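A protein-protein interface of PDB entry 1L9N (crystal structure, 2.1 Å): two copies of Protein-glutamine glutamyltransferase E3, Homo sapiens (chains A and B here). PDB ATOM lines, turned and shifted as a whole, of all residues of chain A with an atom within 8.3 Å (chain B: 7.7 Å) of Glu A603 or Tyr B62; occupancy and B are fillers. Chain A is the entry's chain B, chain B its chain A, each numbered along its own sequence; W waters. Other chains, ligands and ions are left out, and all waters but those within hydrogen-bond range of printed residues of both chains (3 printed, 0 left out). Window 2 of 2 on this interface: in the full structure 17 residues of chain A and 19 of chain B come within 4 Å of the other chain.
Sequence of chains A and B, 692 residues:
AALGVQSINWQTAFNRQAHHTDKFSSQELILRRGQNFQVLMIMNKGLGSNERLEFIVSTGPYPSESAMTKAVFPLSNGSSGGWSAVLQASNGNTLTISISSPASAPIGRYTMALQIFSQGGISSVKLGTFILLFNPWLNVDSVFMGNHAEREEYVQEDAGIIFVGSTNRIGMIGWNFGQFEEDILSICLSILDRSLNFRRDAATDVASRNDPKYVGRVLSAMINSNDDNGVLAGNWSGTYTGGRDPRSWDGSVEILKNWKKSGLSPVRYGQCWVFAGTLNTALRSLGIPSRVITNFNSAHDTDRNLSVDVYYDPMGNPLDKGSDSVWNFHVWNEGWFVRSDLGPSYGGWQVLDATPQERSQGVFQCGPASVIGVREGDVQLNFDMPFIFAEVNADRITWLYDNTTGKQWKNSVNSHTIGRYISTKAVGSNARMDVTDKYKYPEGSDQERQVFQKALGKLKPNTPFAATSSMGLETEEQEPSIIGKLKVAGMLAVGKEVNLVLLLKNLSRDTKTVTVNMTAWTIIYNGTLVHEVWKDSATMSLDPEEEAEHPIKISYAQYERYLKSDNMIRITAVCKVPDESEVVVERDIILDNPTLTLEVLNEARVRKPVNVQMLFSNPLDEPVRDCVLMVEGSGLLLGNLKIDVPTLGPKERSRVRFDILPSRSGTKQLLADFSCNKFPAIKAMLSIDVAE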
ATOM      1  N   GLU A 599      12.579 -18.616 -17.219  1.00  0.00           N
ATOM      2  CA  GLU A 599      12.422 -18.363 -15.794  1.00  0.00           C
ATOM      3  C   GLU A 599      12.929 -19.546 -14.982  1.00  0.00           C
ATOM      4  O   GLU A 599      12.540 -20.685 -15.235  1.00  0.00           O
ATOM      5  CB  GLU A 599      10.952 -18.098 -15.455  1.00  0.00           C
ATOM      6  CG  GLU A 599      10.421 -16.788 -16.007  1.00  0.00           C
ATOM      7  CD  GLU A 599       9.014 -16.474 -15.523  1.00  0.00           C
ATOM      8  OE1 GLU A 599       8.527 -15.354 -15.811  1.00  0.00           O
ATOM      9  OE2 GLU A 599       8.402 -17.346 -14.862  1.00  0.00           O
ATOM     10  N   VAL A 600      13.814 -19.279 -14.024  1.00  0.00           N
ATOM     11  CA  VAL A 600      14.341 -20.339 -13.170  1.00  0.00           C
ATOM     12  C   VAL A 600      13.339 -20.465 -12.040  1.00  0.00           C
ATOM     13  O   VAL A 600      12.859 -19.458 -11.536  1.00  0.00           O
ATOM     14  CB  VAL A 600      15.727 -19.982 -12.584  1.00  0.00           C
ATOM     15  CG1 VAL A 600      16.267 -21.150 -11.790  1.00  0.00           C
ATOM     16  CG2 VAL A 600      16.693 -19.646 -13.698  1.00  0.00           C
ATOM     17  N   LEU A 601      13.008 -21.692 -11.652  1.00  0.00           N
ATOM     18  CA  LEU A 601      12.030 -21.891 -10.591  1.00  0.00           C
ATOM     19  C   LEU A 601      12.596 -22.093  -9.187  1.00  0.00           C
ATOM     20  O   LEU A 601      11.980 -22.761  -8.359  1.00  0.00           O
ATOM     21  CB  LEU A 601      11.093 -23.055 -10.938  1.00  0.00           C
ATOM     22  CG  LEU A 601      10.042 -22.830 -12.035  1.00  0.00           C
ATOM     23  CD1 LEU A 601       9.538 -21.395 -11.981  1.00  0.00           C
ATOM     24  CD2 LEU A 601      10.632 -23.112 -13.389  1.00  0.00           C
ATOM     25  N   ASN A 602      13.758 -21.502  -8.921  1.00  0.00           N
ATOM     26  CA  ASN A 602      14.382 -21.592  -7.606  1.00  0.00           C
ATOM     27  C   ASN A 602      15.746 -20.915  -7.593  1.00  0.00           C
ATOM     28  O   ASN A 602      16.183 -20.363  -8.599  1.00  0.00           O
ATOM     29  CB  ASN A 602      14.545 -23.053  -7.194  1.00  0.00           C
ATOM     30  CG  ASN A 602      14.430 -23.246  -5.698  1.00  0.00           C
ATOM     31  OD1 ASN A 602      15.191 -22.663  -4.923  1.00  0.00           O
ATOM     32  ND2 ASN A 602      13.464 -24.063  -5.279  1.00  0.00           N
ATOM     33  N   GLU A 603      16.405 -20.948  -6.439  1.00  0.00           N
ATOM     34  CA  GLU A 603      17.739 -20.380  -6.296  1.00  0.00           C
ATOM     35  C   GLU A 603      18.687 -21.266  -7.088  1.00  0.00           C
ATOM     36  O   GLU A 603      18.389 -22.432  -7.326  1.00  0.00           O
ATOM     37  CB  GLU A 603      18.189 -20.409  -4.838  1.00  0.00           C
ATOM     38  CG  GLU A 603      17.495 -19.440  -3.925  1.00  0.00           C
ATOM     39  CD  GLU A 603      18.073 -19.482  -2.526  1.00  0.00           C
ATOM     40  OE1 GLU A 603      17.749 -18.580  -1.730  1.00  0.00           O
ATOM     41  OE2 GLU A 603      18.847 -20.420  -2.224  1.00  0.00           O
ATOM     42  N   ALA A 604      19.834 -20.720  -7.472  1.00  0.00           N
ATOM     43  CA  ALA A 604      20.825 -21.485  -8.220  1.00  0.00           C
ATOM     44  C   ALA A 604      22.091 -21.678  -7.394  1.00  0.00           C
ATOM     45  O   ALA A 604      22.678 -20.714  -6.912  1.00  0.00           O
ATOM     46  CB  ALA A 604      21.162 -20.777  -9.527  1.00  0.00           C
ATOM     47  N   ARG A 605      22.502 -22.930  -7.229  1.00  0.00           N
ATOM     48  CA  ARG A 605      23.713 -23.248  -6.481  1.00  0.00           C
ATOM     49  C   ARG A 605      24.521 -24.321  -7.194  1.00  0.00           C
ATOM     50  O   ARG A 605      23.967 -25.173  -7.890  1.00  0.00           O
ATOM     51  CB  ARG A 605      23.375 -23.732  -5.072  1.00  0.00           C
ATOM     52  CG  ARG A 605      22.641 -22.711  -4.239  1.00  0.00           C
ATOM     53  CD  ARG A 605      22.610 -23.128  -2.788  1.00  0.00           C
ATOM     54  NE  ARG A 605      21.755 -22.251  -1.999  1.00  0.00           N
ATOM     55  CZ  ARG A 605      21.668 -22.300  -0.675  1.00  0.00           C
ATOM     56  NH1 ARG A 605      22.393 -23.187  -0.001  1.00  0.00           N
ATOM     57  NH2 ARG A 605      20.860 -21.469  -0.025  1.00  0.00           N
ATOM     58  N   VAL A 606      25.834 -24.276  -7.003  1.00  0.00           N
ATOM     59  CA  VAL A 606      26.736 -25.234  -7.627  1.00  0.00           C
ATOM     60  C   VAL A 606      26.336 -26.688  -7.396  1.00  0.00           C
ATOM     61  O   VAL A 606      26.029 -27.088  -6.275  1.00  0.00           O
ATOM     62  CB  VAL A 606      28.183 -25.040  -7.125  1.00  0.00           C
ATOM     63  CG1 VAL A 606      29.098 -26.066  -7.771  1.00  0.00           C
ATOM     64  CG2 VAL A 606      28.658 -23.624  -7.441  1.00  0.00           C
ATOM     65  N   LYS A 608      23.768 -28.225  -7.878  1.00  0.00           N
ATOM     66  CA  LYS A 608      22.380 -28.453  -7.509  1.00  0.00           C
ATOM     67  C   LYS A 608      21.481 -28.236  -8.731  1.00  0.00           C
ATOM     68  O   LYS A 608      21.374 -27.124  -9.247  1.00  0.00           O
ATOM     69  CB  LYS A 608      21.986 -27.500  -6.381  1.00  0.00           C
ATOM     70  CG  LYS A 608      20.691 -27.872  -5.685  1.00  0.00           C
ATOM     71  CD  LYS A 608      20.315 -26.840  -4.627  1.00  0.00           C
ATOM     72  CE  LYS A 608      19.166 -27.340  -3.756  1.00  0.00           C
ATOM     73  NZ  LYS A 608      18.027 -27.828  -4.583  1.00  0.00           N
ATOM     74  N   PRO A 609      20.826 -29.303  -9.215  1.00  0.00           N
ATOM     75  CA  PRO A 609      19.945 -29.184 -10.379  1.00  0.00           C
ATOM     76  C   PRO A 609      18.787 -28.242 -10.088  1.00  0.00           C
ATOM     77  O   PRO A 609      18.187 -28.306  -9.017  1.00  0.00           O
ATOM     78  CB  PRO A 609      19.462 -30.617 -10.599  1.00  0.00           C
ATOM     79  CG  PRO A 609      20.580 -31.448 -10.042  1.00  0.00           C
ATOM     80  CD  PRO A 609      20.923 -30.705  -8.777  1.00  0.00           C
ATOM     81  N   VAL A 610      18.482 -27.360 -11.033  1.00  0.00           N
ATOM     82  CA  VAL A 610      17.369 -26.443 -10.850  1.00  0.00           C
ATOM     83  C   VAL A 610      16.534 -26.369 -12.127  1.00  0.00           C
ATOM     84  O   VAL A 610      17.071 -26.243 -13.232  1.00  0.00           O
ATOM     85  CB  VAL A 610      17.854 -25.034 -10.459  1.00  0.00           C
ATOM     86  CG1 VAL A 610      18.749 -24.463 -11.546  1.00  0.00           C
ATOM     87  CG2 VAL A 610      16.650 -24.131 -10.201  1.00  0.00           C
ATOM     88  N   ASN A 611      15.218 -26.453 -11.959  1.00  0.00           N
ATOM     89  CA  ASN A 611      14.295 -26.425 -13.082  1.00  0.00           C
ATOM     90  C   ASN A 611      14.116 -25.018 -13.643  1.00  0.00           C
ATOM     91  O   ASN A 611      14.137 -24.040 -12.903  1.00  0.00           O
ATOM     92  CB  ASN A 611      12.929 -26.980 -12.660  1.00  0.00           C
ATOM     93  CG  ASN A 611      12.102 -27.445 -13.845  1.00  0.00           C
ATOM     94  OD1 ASN A 611      10.879 -27.306 -13.863  1.00  0.00           O
ATOM     95  ND2 ASN A 611      12.771 -28.016 -14.841  1.00  0.00           N
ATOM     96  N   GLN A 613      11.816 -22.786 -16.866  1.00  0.00           N
ATOM     97  CA  GLN A 613      10.684 -22.878 -17.784  1.00  0.00           C
ATOM     98  C   GLN A 613      10.786 -21.884 -18.933  1.00  0.00           C
ATOM     99  O   GLN A 613      11.182 -20.732 -18.751  1.00  0.00           O
ATOM    100  CB  GLN A 613       9.352 -22.675 -17.046  1.00  0.00           C
ATOM    101  CG  GLN A 613       9.272 -21.420 -16.180  1.00  0.00           C
ATOM    102  CD  GLN A 613       7.900 -21.247 -15.536  1.00  0.00           C
ATOM    103  OE1 GLN A 613       7.256 -22.223 -15.145  1.00  0.00           O
ATOM    104  NE2 GLN A 613       7.457 -20.002 -15.414  1.00  0.00           N
ATOM    105  N   ILE A 660      18.919 -27.166 -15.520  1.00  0.00           N
ATOM    106  CA  ILE A 660      20.266 -26.707 -15.821  1.00  0.00           C
ATOM    107  C   ILE A 660      21.046 -27.179 -14.592  1.00  0.00           C
ATOM    108  O   ILE A 660      20.449 -27.474 -13.554  1.00  0.00           O
ATOM    109  CB  ILE A 660      20.370 -25.158 -15.952  1.00  0.00           C
ATOM    110  CG1 ILE A 660      19.966 -24.486 -14.640  1.00  0.00           C
ATOM    111  CG2 ILE A 660      19.515 -24.680 -17.117  1.00  0.00           C
ATOM    112  CD1 ILE A 660      20.139 -22.979 -14.643  1.00  0.00           C
ATOM    113  N   PRO A 662      24.208 -25.813 -12.483  1.00  0.00           N
ATOM    114  CA  PRO A 662      25.285 -24.868 -12.178  1.00  0.00           C
ATOM    115  C   PRO A 662      26.563 -25.599 -11.764  1.00  0.00           C
ATOM    116  O   PRO A 662      26.518 -26.523 -10.950  1.00  0.00           O
ATOM    117  CB  PRO A 662      24.693 -24.035 -11.047  1.00  0.00           C
ATOM    118  CG  PRO A 662      23.225 -24.033 -11.374  1.00  0.00           C
ATOM    119  CD  PRO A 662      22.986 -25.475 -11.733  1.00  0.00           C
ATOM    120  N   ILE A 688      21.697 -15.321 -14.388  1.00  0.00           N
ATOM    121  CA  ILE A 688      21.452 -16.109 -13.185  1.00  0.00           C
ATOM    122  C   ILE A 688      22.606 -16.060 -12.194  1.00  0.00           C
ATOM    123  O   ILE A 688      23.757 -16.337 -12.553  1.00  0.00           O
ATOM    124  CB  ILE A 688      21.196 -17.601 -13.525  1.00  0.00           C
ATOM    125  CG1 ILE A 688      20.051 -17.729 -14.533  1.00  0.00           C
ATOM    126  CG2 ILE A 688      20.868 -18.370 -12.258  1.00  0.00           C
ATOM    127  CD1 ILE A 688      19.886 -19.125 -15.082  1.00  0.00           C
ATOM    128  N   ASP A 689      22.294 -15.718 -10.946  1.00  0.00           N
ATOM    129  CA  ASP A 689      23.311 -15.663  -9.897  1.00  0.00           C
ATOM    130  C   ASP A 689      23.428 -17.036  -9.241  1.00  0.00           C
ATOM    131  O   ASP A 689      22.493 -17.516  -8.602  1.00  0.00           O
ATOM    132  CB  ASP A 689      22.957 -14.606  -8.846  1.00  0.00           C
ATOM    133  CG  ASP A 689      23.096 -13.192  -9.377  1.00  0.00           C
ATOM    134  OD1 ASP A 689      24.203 -12.830  -9.834  1.00  0.00           O
ATOM    135  OD2 ASP A 689      22.098 -12.439  -9.339  1.00  0.00           O
ATOM    136  N   VAL A 690      24.582 -17.666  -9.428  1.00  0.00           N
ATOM    137  CA  VAL A 690      24.844 -18.986  -8.874  1.00  0.00           C
ATOM    138  C   VAL A 690      25.675 -18.876  -7.605  1.00  0.00           C
ATOM    139  O   VAL A 690      26.808 -18.402  -7.641  1.00  0.00           O
ATOM    140  CB  VAL A 690      25.615 -19.865  -9.874  1.00  0.00           C
ATOM    141  CG1 VAL A 690      25.880 -21.242  -9.259  1.00  0.00           C
ATOM    142  CG2 VAL A 690      24.819 -19.993 -11.173  1.00  0.00           C
ATOM    143  N   ALA A 691      25.108 -19.324  -6.488  1.00  0.00           N
ATOM    144  CA  ALA A 691      25.798 -19.277  -5.207  1.00  0.00           C
ATOM    145  C   ALA A 691      26.746 -20.459  -5.077  1.00  0.00           C
ATOM    146  O   ALA A 691      26.621 -21.453  -5.798  1.00  0.00           O
ATOM    147  CB  ALA A 691      24.786 -19.291  -4.058  1.00  0.00           C
ATOM    148  N   SER B  58      -0.865 -15.925 -10.379  1.00  0.00           N
ATOM    149  CA  SER B  58       0.309 -16.576  -9.820  1.00  0.00           C
ATOM    150  C   SER B  58       0.624 -16.100  -8.405  1.00  0.00           C
ATOM    151  O   SER B  58       0.353 -14.948  -8.045  1.00  0.00           O
ATOM    152  CB  SER B  58       1.509 -16.318 -10.735  1.00  0.00           C
ATOM    153  OG  SER B  58       1.659 -14.930 -10.986  1.00  0.00           O
ATOM    154  N   THR B  59       1.204 -16.994  -7.605  1.00  0.00           N
ATOM    155  CA  THR B  59       1.571 -16.657  -6.235  1.00  0.00           C
ATOM    156  C   THR B  59       2.954 -17.201  -5.905  1.00  0.00           C
ATOM    157  O   THR B  59       3.344 -18.274  -6.381  1.00  0.00           O
ATOM    158  CB  THR B  59       0.549 -17.227  -5.214  1.00  0.00           C
ATOM    159  OG1 THR B  59       0.948 -16.853  -3.888  1.00  0.00           O
ATOM    160  CG2 THR B  59       0.465 -18.761  -5.315  1.00  0.00           C
ATOM    161  N   GLY B  60       3.696 -16.458  -5.093  1.00  0.00           N
ATOM    162  CA  GLY B  60       5.028 -16.895  -4.719  1.00  0.00           C
ATOM    163  C   GLY B  60       6.104 -16.350  -5.642  1.00  0.00           C
ATOM    164  O   GLY B  60       5.792 -15.746  -6.666  1.00  0.00           O
ATOM    165  N   PRO B  61       7.386 -16.544  -5.305  1.00  0.00           N
ATOM    166  CA  PRO B  61       8.488 -16.048  -6.137  1.00  0.00           C
ATOM    167  C   PRO B  61       8.865 -16.933  -7.331  1.00  0.00           C
ATOM    168  O   PRO B  61       9.669 -16.531  -8.174  1.00  0.00           O
ATOM    169  CB  PRO B  61       9.629 -15.912  -5.136  1.00  0.00           C
ATOM    170  CG  PRO B  61       9.381 -17.089  -4.224  1.00  0.00           C
ATOM    171  CD  PRO B  61       7.884 -17.029  -4.003  1.00  0.00           C
ATOM    172  N   TYR B  62       8.286 -18.131  -7.406  1.00  0.00           N
ATOM    173  CA  TYR B  62       8.584 -19.056  -8.502  1.00  0.00           C
ATOM    174  C   TYR B  62       7.313 -19.753  -9.007  1.00  0.00           C
ATOM    175  O   TYR B  62       7.214 -20.980  -8.982  1.00  0.00           O
ATOM    176  CB  TYR B  62       9.595 -20.110  -8.030  1.00  0.00           C
ATOM    177  CG  TYR B  62      10.877 -19.535  -7.466  1.00  0.00           C
ATOM    178  CD1 TYR B  62      11.767 -18.828  -8.275  1.00  0.00           C
ATOM    179  CD2 TYR B  62      11.192 -19.684  -6.112  1.00  0.00           C
ATOM    180  CE1 TYR B  62      12.943 -18.279  -7.750  1.00  0.00           C
ATOM    181  CE2 TYR B  62      12.364 -19.140  -5.575  1.00  0.00           C
ATOM    182  CZ  TYR B  62      13.232 -18.441  -6.399  1.00  0.00           C
ATOM    183  OH  TYR B  62      14.378 -17.900  -5.868  1.00  0.00           O
ATOM    184  N   PRO B  63       6.332 -18.975  -9.490  1.00  0.00           N
ATOM    185  CA  PRO B  63       5.065 -19.517  -9.996  1.00  0.00           C
ATOM    186  C   PRO B  63       5.234 -20.464 -11.178  1.00  0.00           C
ATOM    187  O   PRO B  63       5.940 -20.153 -12.131  1.00  0.00           O
ATOM    188  CB  PRO B  63       4.281 -18.261 -10.404  1.00  0.00           C
ATOM    189  CG  PRO B  63       4.889 -17.178  -9.588  1.00  0.00           C
ATOM    190  CD  PRO B  63       6.356 -17.509  -9.627  1.00  0.00           C
ATOM    191  N   SER B  64       4.582 -21.618 -11.111  1.00  0.00           N
ATOM    192  CA  SER B  64       4.642 -22.582 -12.203  1.00  0.00           C
ATOM    193  C   SER B  64       3.330 -23.344 -12.253  1.00  0.00           C
ATOM    194  O   SER B  64       2.737 -23.663 -11.217  1.00  0.00           O
ATOM    195  CB  SER B  64       5.808 -23.562 -12.022  1.00  0.00           C
ATOM    196  OG  SER B  64       5.594 -24.431 -10.926  1.00  0.00           O
ATOM    197  N   GLU B  65       2.880 -23.640 -13.466  1.00  0.00           N
ATOM    198  CA  GLU B  65       1.630 -24.349 -13.643  1.00  0.00           C
ATOM    199  C   GLU B  65       1.666 -25.750 -13.043  1.00  0.00           C
ATOM    200  O   GLU B  65       0.664 -26.217 -12.496  1.00  0.00           O
ATOM    201  CB  GLU B  65       1.273 -24.417 -15.131  1.00  0.00           C
ATOM    202  CG  GLU B  65       1.286 -23.065 -15.833  1.00  0.00           C
ATOM    203  CD  GLU B  65       0.488 -23.074 -17.127  1.00  0.00           C
ATOM    204  OE1 GLU B  65       0.723 -22.193 -17.982  1.00  0.00           O
ATOM    205  OE2 GLU B  65      -0.384 -23.956 -17.283  1.00  0.00           O
ATOM    206  N   ALA B  67       3.207 -26.748 -10.405  1.00  0.00           N
ATOM    207  CA  ALA B  67       3.089 -26.679  -8.949  1.00  0.00           C
ATOM    208  C   ALA B  67       1.755 -26.078  -8.503  1.00  0.00           C
ATOM    209  O   ALA B  67       1.479 -25.983  -7.309  1.00  0.00           O
ATOM    210  CB  ALA B  67       4.240 -25.865  -8.372  1.00  0.00           C
ATOM    211  N   THR B  69       0.982 -23.122  -8.633  1.00  0.00           N
ATOM    212  CA  THR B  69       1.203 -21.778  -8.118  1.00  0.00           C
ATOM    213  C   THR B  69       1.057 -20.762  -9.238  1.00  0.00           C
ATOM    214  O   THR B  69       1.382 -19.585  -9.079  1.00  0.00           O
ATOM    215  CB  THR B  69       2.596 -21.635  -7.465  1.00  0.00           C
ATOM    216  OG1 THR B  69       3.602 -22.100  -8.368  1.00  0.00           O
ATOM    217  CG2 THR B  69       2.660 -22.439  -6.171  1.00  0.00           C
ATOM    218  N   LYS B  70       0.557 -21.237 -10.373  1.00  0.00           N
ATOM    219  CA  LYS B  70       0.319 -20.410 -11.552  1.00  0.00           C
ATOM    220  C   LYS B  70      -0.690 -21.113 -12.450  1.00  0.00           C
ATOM    221  O   LYS B  70      -0.623 -22.334 -12.629  1.00  0.00           O
ATOM    222  CB  LYS B  70       1.613 -20.190 -12.343  1.00  0.00           C
ATOM    223  CG  LYS B  70       1.419 -19.397 -13.636  1.00  0.00           C
ATOM    224  CD  LYS B  70       2.714 -19.312 -14.425  1.00  0.00           C
ATOM    225  CE  LYS B  70       2.564 -18.467 -15.681  1.00  0.00           C
ATOM    226  NZ  LYS B  70       3.855 -18.327 -16.423  1.00  0.00           N
ATOM    227  N   PHE B 198       9.993 -22.142   3.875  1.00  0.00           N
ATOM    228  CA  PHE B 198      10.061 -21.192   2.768  1.00  0.00           C
ATOM    229  C   PHE B 198      11.488 -20.808   2.393  1.00  0.00           C
ATOM    230  O   PHE B 198      11.798 -20.644   1.216  1.00  0.00           O
ATOM    231  CB  PHE B 198       9.253 -19.932   3.101  1.00  0.00           C
ATOM    232  CG  PHE B 198       9.239 -18.908   1.997  1.00  0.00           C
ATOM    233  CD1 PHE B 198      10.172 -17.870   1.974  1.00  0.00           C
ATOM    234  CD2 PHE B 198       8.296 -18.981   0.974  1.00  0.00           C
ATOM    235  CE1 PHE B 198      10.165 -16.919   0.951  1.00  0.00           C
ATOM    236  CE2 PHE B 198       8.279 -18.035  -0.056  1.00  0.00           C
ATOM    237  CZ  PHE B 198       9.221 -16.998  -0.064  1.00  0.00           C
ATOM    238  N   ARG B 199      12.349 -20.657   3.394  1.00  0.00           N
ATOM    239  CA  ARG B 199      13.739 -20.299   3.161  1.00  0.00           C
ATOM    240  C   ARG B 199      14.507 -21.469   2.565  1.00  0.00           C
ATOM    241  O   ARG B 199      15.479 -21.288   1.835  1.00  0.00           O
ATOM    242  CB  ARG B 199      14.393 -19.865   4.473  1.00  0.00           C
ATOM    243  CG  ARG B 199      14.032 -18.460   4.898  1.00  0.00           C
ATOM    244  CD  ARG B 199      14.670 -18.119   6.230  1.00  0.00           C
ATOM    245  NE  ARG B 199      13.734 -18.287   7.332  1.00  0.00           N
ATOM    246  CZ  ARG B 199      14.075 -18.254   8.618  1.00  0.00           C
ATOM    247  NH1 ARG B 199      15.342 -18.063   8.966  1.00  0.00           N
ATOM    248  NH2 ARG B 199      13.145 -18.409   9.559  1.00  0.00           N
ATOM    249  N   ARG B 200      14.058 -22.675   2.883  1.00  0.00           N
ATOM    250  CA  ARG B 200      14.686 -23.883   2.384  1.00  0.00           C
ATOM    251  C   ARG B 200      14.333 -24.085   0.913  1.00  0.00           C
ATOM    252  O   ARG B 200      15.201 -24.347   0.084  1.00  0.00           O
ATOM    253  CB  ARG B 200      14.209 -25.071   3.212  1.00  0.00           C
ATOM    254  CG  ARG B 200      15.052 -26.322   3.101  1.00  0.00           C
ATOM    255  CD  ARG B 200      15.034 -27.040   4.446  1.00  0.00           C
ATOM    256  NE  ARG B 200      13.672 -27.141   4.969  1.00  0.00           N
ATOM    257  CZ  ARG B 200      13.337 -26.912   6.236  1.00  0.00           C
ATOM    258  NH1 ARG B 200      14.266 -26.570   7.122  1.00  0.00           N
ATOM    259  NH2 ARG B 200      12.070 -27.008   6.617  1.00  0.00           N
ATOM    260  N   ASP B 201      13.052 -23.952   0.595  1.00  0.00           N
ATOM    261  CA  ASP B 201      12.574 -24.127  -0.771  1.00  0.00           C
ATOM    262  C   ASP B 201      11.257 -23.368  -0.920  1.00  0.00           C
ATOM    263  O   ASP B 201      10.191 -23.901  -0.615  1.00  0.00           O
ATOM    264  CB  ASP B 201      12.355 -25.617  -1.059  1.00  0.00           C
ATOM    265  CG  ASP B 201      12.042 -25.896  -2.518  1.00  0.00           C
ATOM    266  OD1 ASP B 201      11.640 -24.965  -3.243  1.00  0.00           O
ATOM    267  OD2 ASP B 201      12.188 -27.059  -2.938  1.00  0.00           O
ATOM    268  N   ALA B 202      11.343 -22.122  -1.382  1.00  0.00           N
ATOM    269  CA  ALA B 202      10.170 -21.272  -1.565  1.00  0.00           C
ATOM    270  C   ALA B 202       9.182 -21.813  -2.595  1.00  0.00           C
ATOM    271  O   ALA B 202       7.974 -21.724  -2.399  1.00  0.00           O
ATOM    272  CB  ALA B 202      10.604 -19.866  -1.957  1.00  0.00           C
ATOM    273  N   ALA B 203       9.688 -22.373  -3.688  1.00  0.00           N
ATOM    274  CA  ALA B 203       8.808 -22.908  -4.729  1.00  0.00           C
ATOM    275  C   ALA B 203       7.916 -24.023  -4.179  1.00  0.00           C
ATOM    276  O   ALA B 203       6.704 -24.037  -4.407  1.00  0.00           O
ATOM    277  CB  ALA B 203       9.637 -23.433  -5.910  1.00  0.00           C
ATOM    278  N   THR B 204       8.528 -24.954  -3.459  1.00  0.00           N
ATOM    279  CA  THR B 204       7.808 -26.082  -2.872  1.00  0.00           C
ATOM    280  C   THR B 204       6.881 -25.638  -1.749  1.00  0.00           C
ATOM    281  O   THR B 204       5.740 -26.089  -1.655  1.00  0.00           O
ATOM    282  CB  THR B 204       8.806 -27.136  -2.332  1.00  0.00           C
ATOM    283  OG1 THR B 204       9.453 -27.775  -3.440  1.00  0.00           O
ATOM    284  CG2 THR B 204       8.096 -28.186  -1.483  1.00  0.00           C
ATOM    285  N   VAL B 206       5.356 -22.659  -1.165  1.00  0.00           N
ATOM    286  CA  VAL B 206       4.153 -22.009  -1.667  1.00  0.00           C
ATOM    287  C   VAL B 206       3.157 -23.004  -2.253  1.00  0.00           C
ATOM    288  O   VAL B 206       1.956 -22.858  -2.074  1.00  0.00           O
ATOM    289  CB  VAL B 206       4.485 -20.932  -2.725  1.00  0.00           C
ATOM    290  CG1 VAL B 206       3.194 -20.366  -3.321  1.00  0.00           C
ATOM    291  CG2 VAL B 206       5.288 -19.813  -2.081  1.00  0.00           C
ATOM    292  N   ALA B 207       3.656 -24.022  -2.943  1.00  0.00           N
ATOM    293  CA  ALA B 207       2.784 -25.027  -3.544  1.00  0.00           C
ATOM    294  C   ALA B 207       2.066 -25.860  -2.477  1.00  0.00           C
ATOM    295  O   ALA B 207       0.958 -26.346  -2.694  1.00  0.00           O
ATOM    296  CB  ALA B 207       3.604 -25.944  -4.461  1.00  0.00           C
HETATM  297  O   HOH W   1      13.707 -21.106  -2.441  1.00  0.00           O
HETATM  298  O   HOH W   2       4.455 -22.328 -15.994  1.00  0.00           O
HETATM  299  O   HOH W   3       5.632 -17.532 -14.592  1.00  0.00           O
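Val A600 touches Tyr B62 (O to CD1, 3.5 Å). CD1 of Tyr B62 touches C of Leu A601, at 3.5 Å. CD1 of Leu A601 touches O of Pro B63, 3.8 Å away. CB of Ala B203 touches O of Leu A601 (3.5 Å). N of Asn A602 touches CD1 of Tyr B62, at 3.4 Å. Asn A602 touches Ala B203. OH of Tyr B62 touches N of Glu A603 (3.7 Å). Pro B63 touches Gln A613.
No position is printed for both chains. Of the 10 pairs that touch across the chains among the printed residues, none has its exchanged pair printed and touching as well.
Of the 20 printed residues of chain B, 5 touch a printed residue of chain A. Hydrophobic or aromatic side chains of chain B that line the printed part of chain A: Tyr B62 and Ala B203. Of the 19 printed residues of chain A, 5 touch a printed residue of chain B. Among the printed residues, no Asp or Glu carboxylate lies within 4 Å of a Lys or Arg side-chain nitrogen of the other chain.
Of the printed residues of chain B, Val A600 touches Tyr B62. Of the printed residues of chain B, Asn A602 touches Tyr B62 (3.4 Å), Asp B201 (2.9 Å) and Ala B203 (3.9 Å). Of chain B, only Tyr B62 (3.7 Å) comes within 4 Å of Glu A603. Ser B58 touches none of the printed residues of chain A. No residue of chain A comes within 4 Å of Pro B61. Of chain A, only Val A600 (3.5 Å), Leu A601 (3.5 Å), Asn A602 (3.4 Å) and Glu A603 (3.7 Å) come within 4 Å of Tyr B62. Pro B63 touches just these residues of chain A: Leu A601 (3.8 Å) and Gln A613 (3.6 Å). Of the printed residues of chain A, Ser B64 touches Gln A613. Printed residues of chain A within 4 Å of Asp B201: Asn A602 (2.9 Å). The nearest residue of chain B that does not touch Glu A603 is Arg B199 (5.0 Å). The nearest printed residue of chain B that does not touch Gln A613 is Lys B70 (4.1 Å).
Water W3 lies within hydrogen-bond range of the side-chain amino group (NZ) of Lys B70, the side-chain carboxylate (OE2) of Glu A599 and the side-chain amide nitrogen (NE2) of Gln A613. Water W2 bridges the side-chain amide oxygen (OE1) of Gln A613 and the backbone NH (N) of Glu B65.
The backbone NH (N) of Leu A601 is in hydrogen-bond range of the backbone carbonyl oxygen (O) of Asn A611 (2.9 Å). The backbone carbonyl oxygen of Ser B64 lies within hydrogen-bond range of the backbone NH of Lys B70. The backbone carbonyl oxygen (O) of Glu A599 lies within hydrogen-bond range of the backbone NH (N) of Gln A613 (2.8 Å).
The side-chain carboxylate of Asp B201 lies within hydrogen-bond range of the side-chain amide nitrogen of Asn A602, at 2.9 Å.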
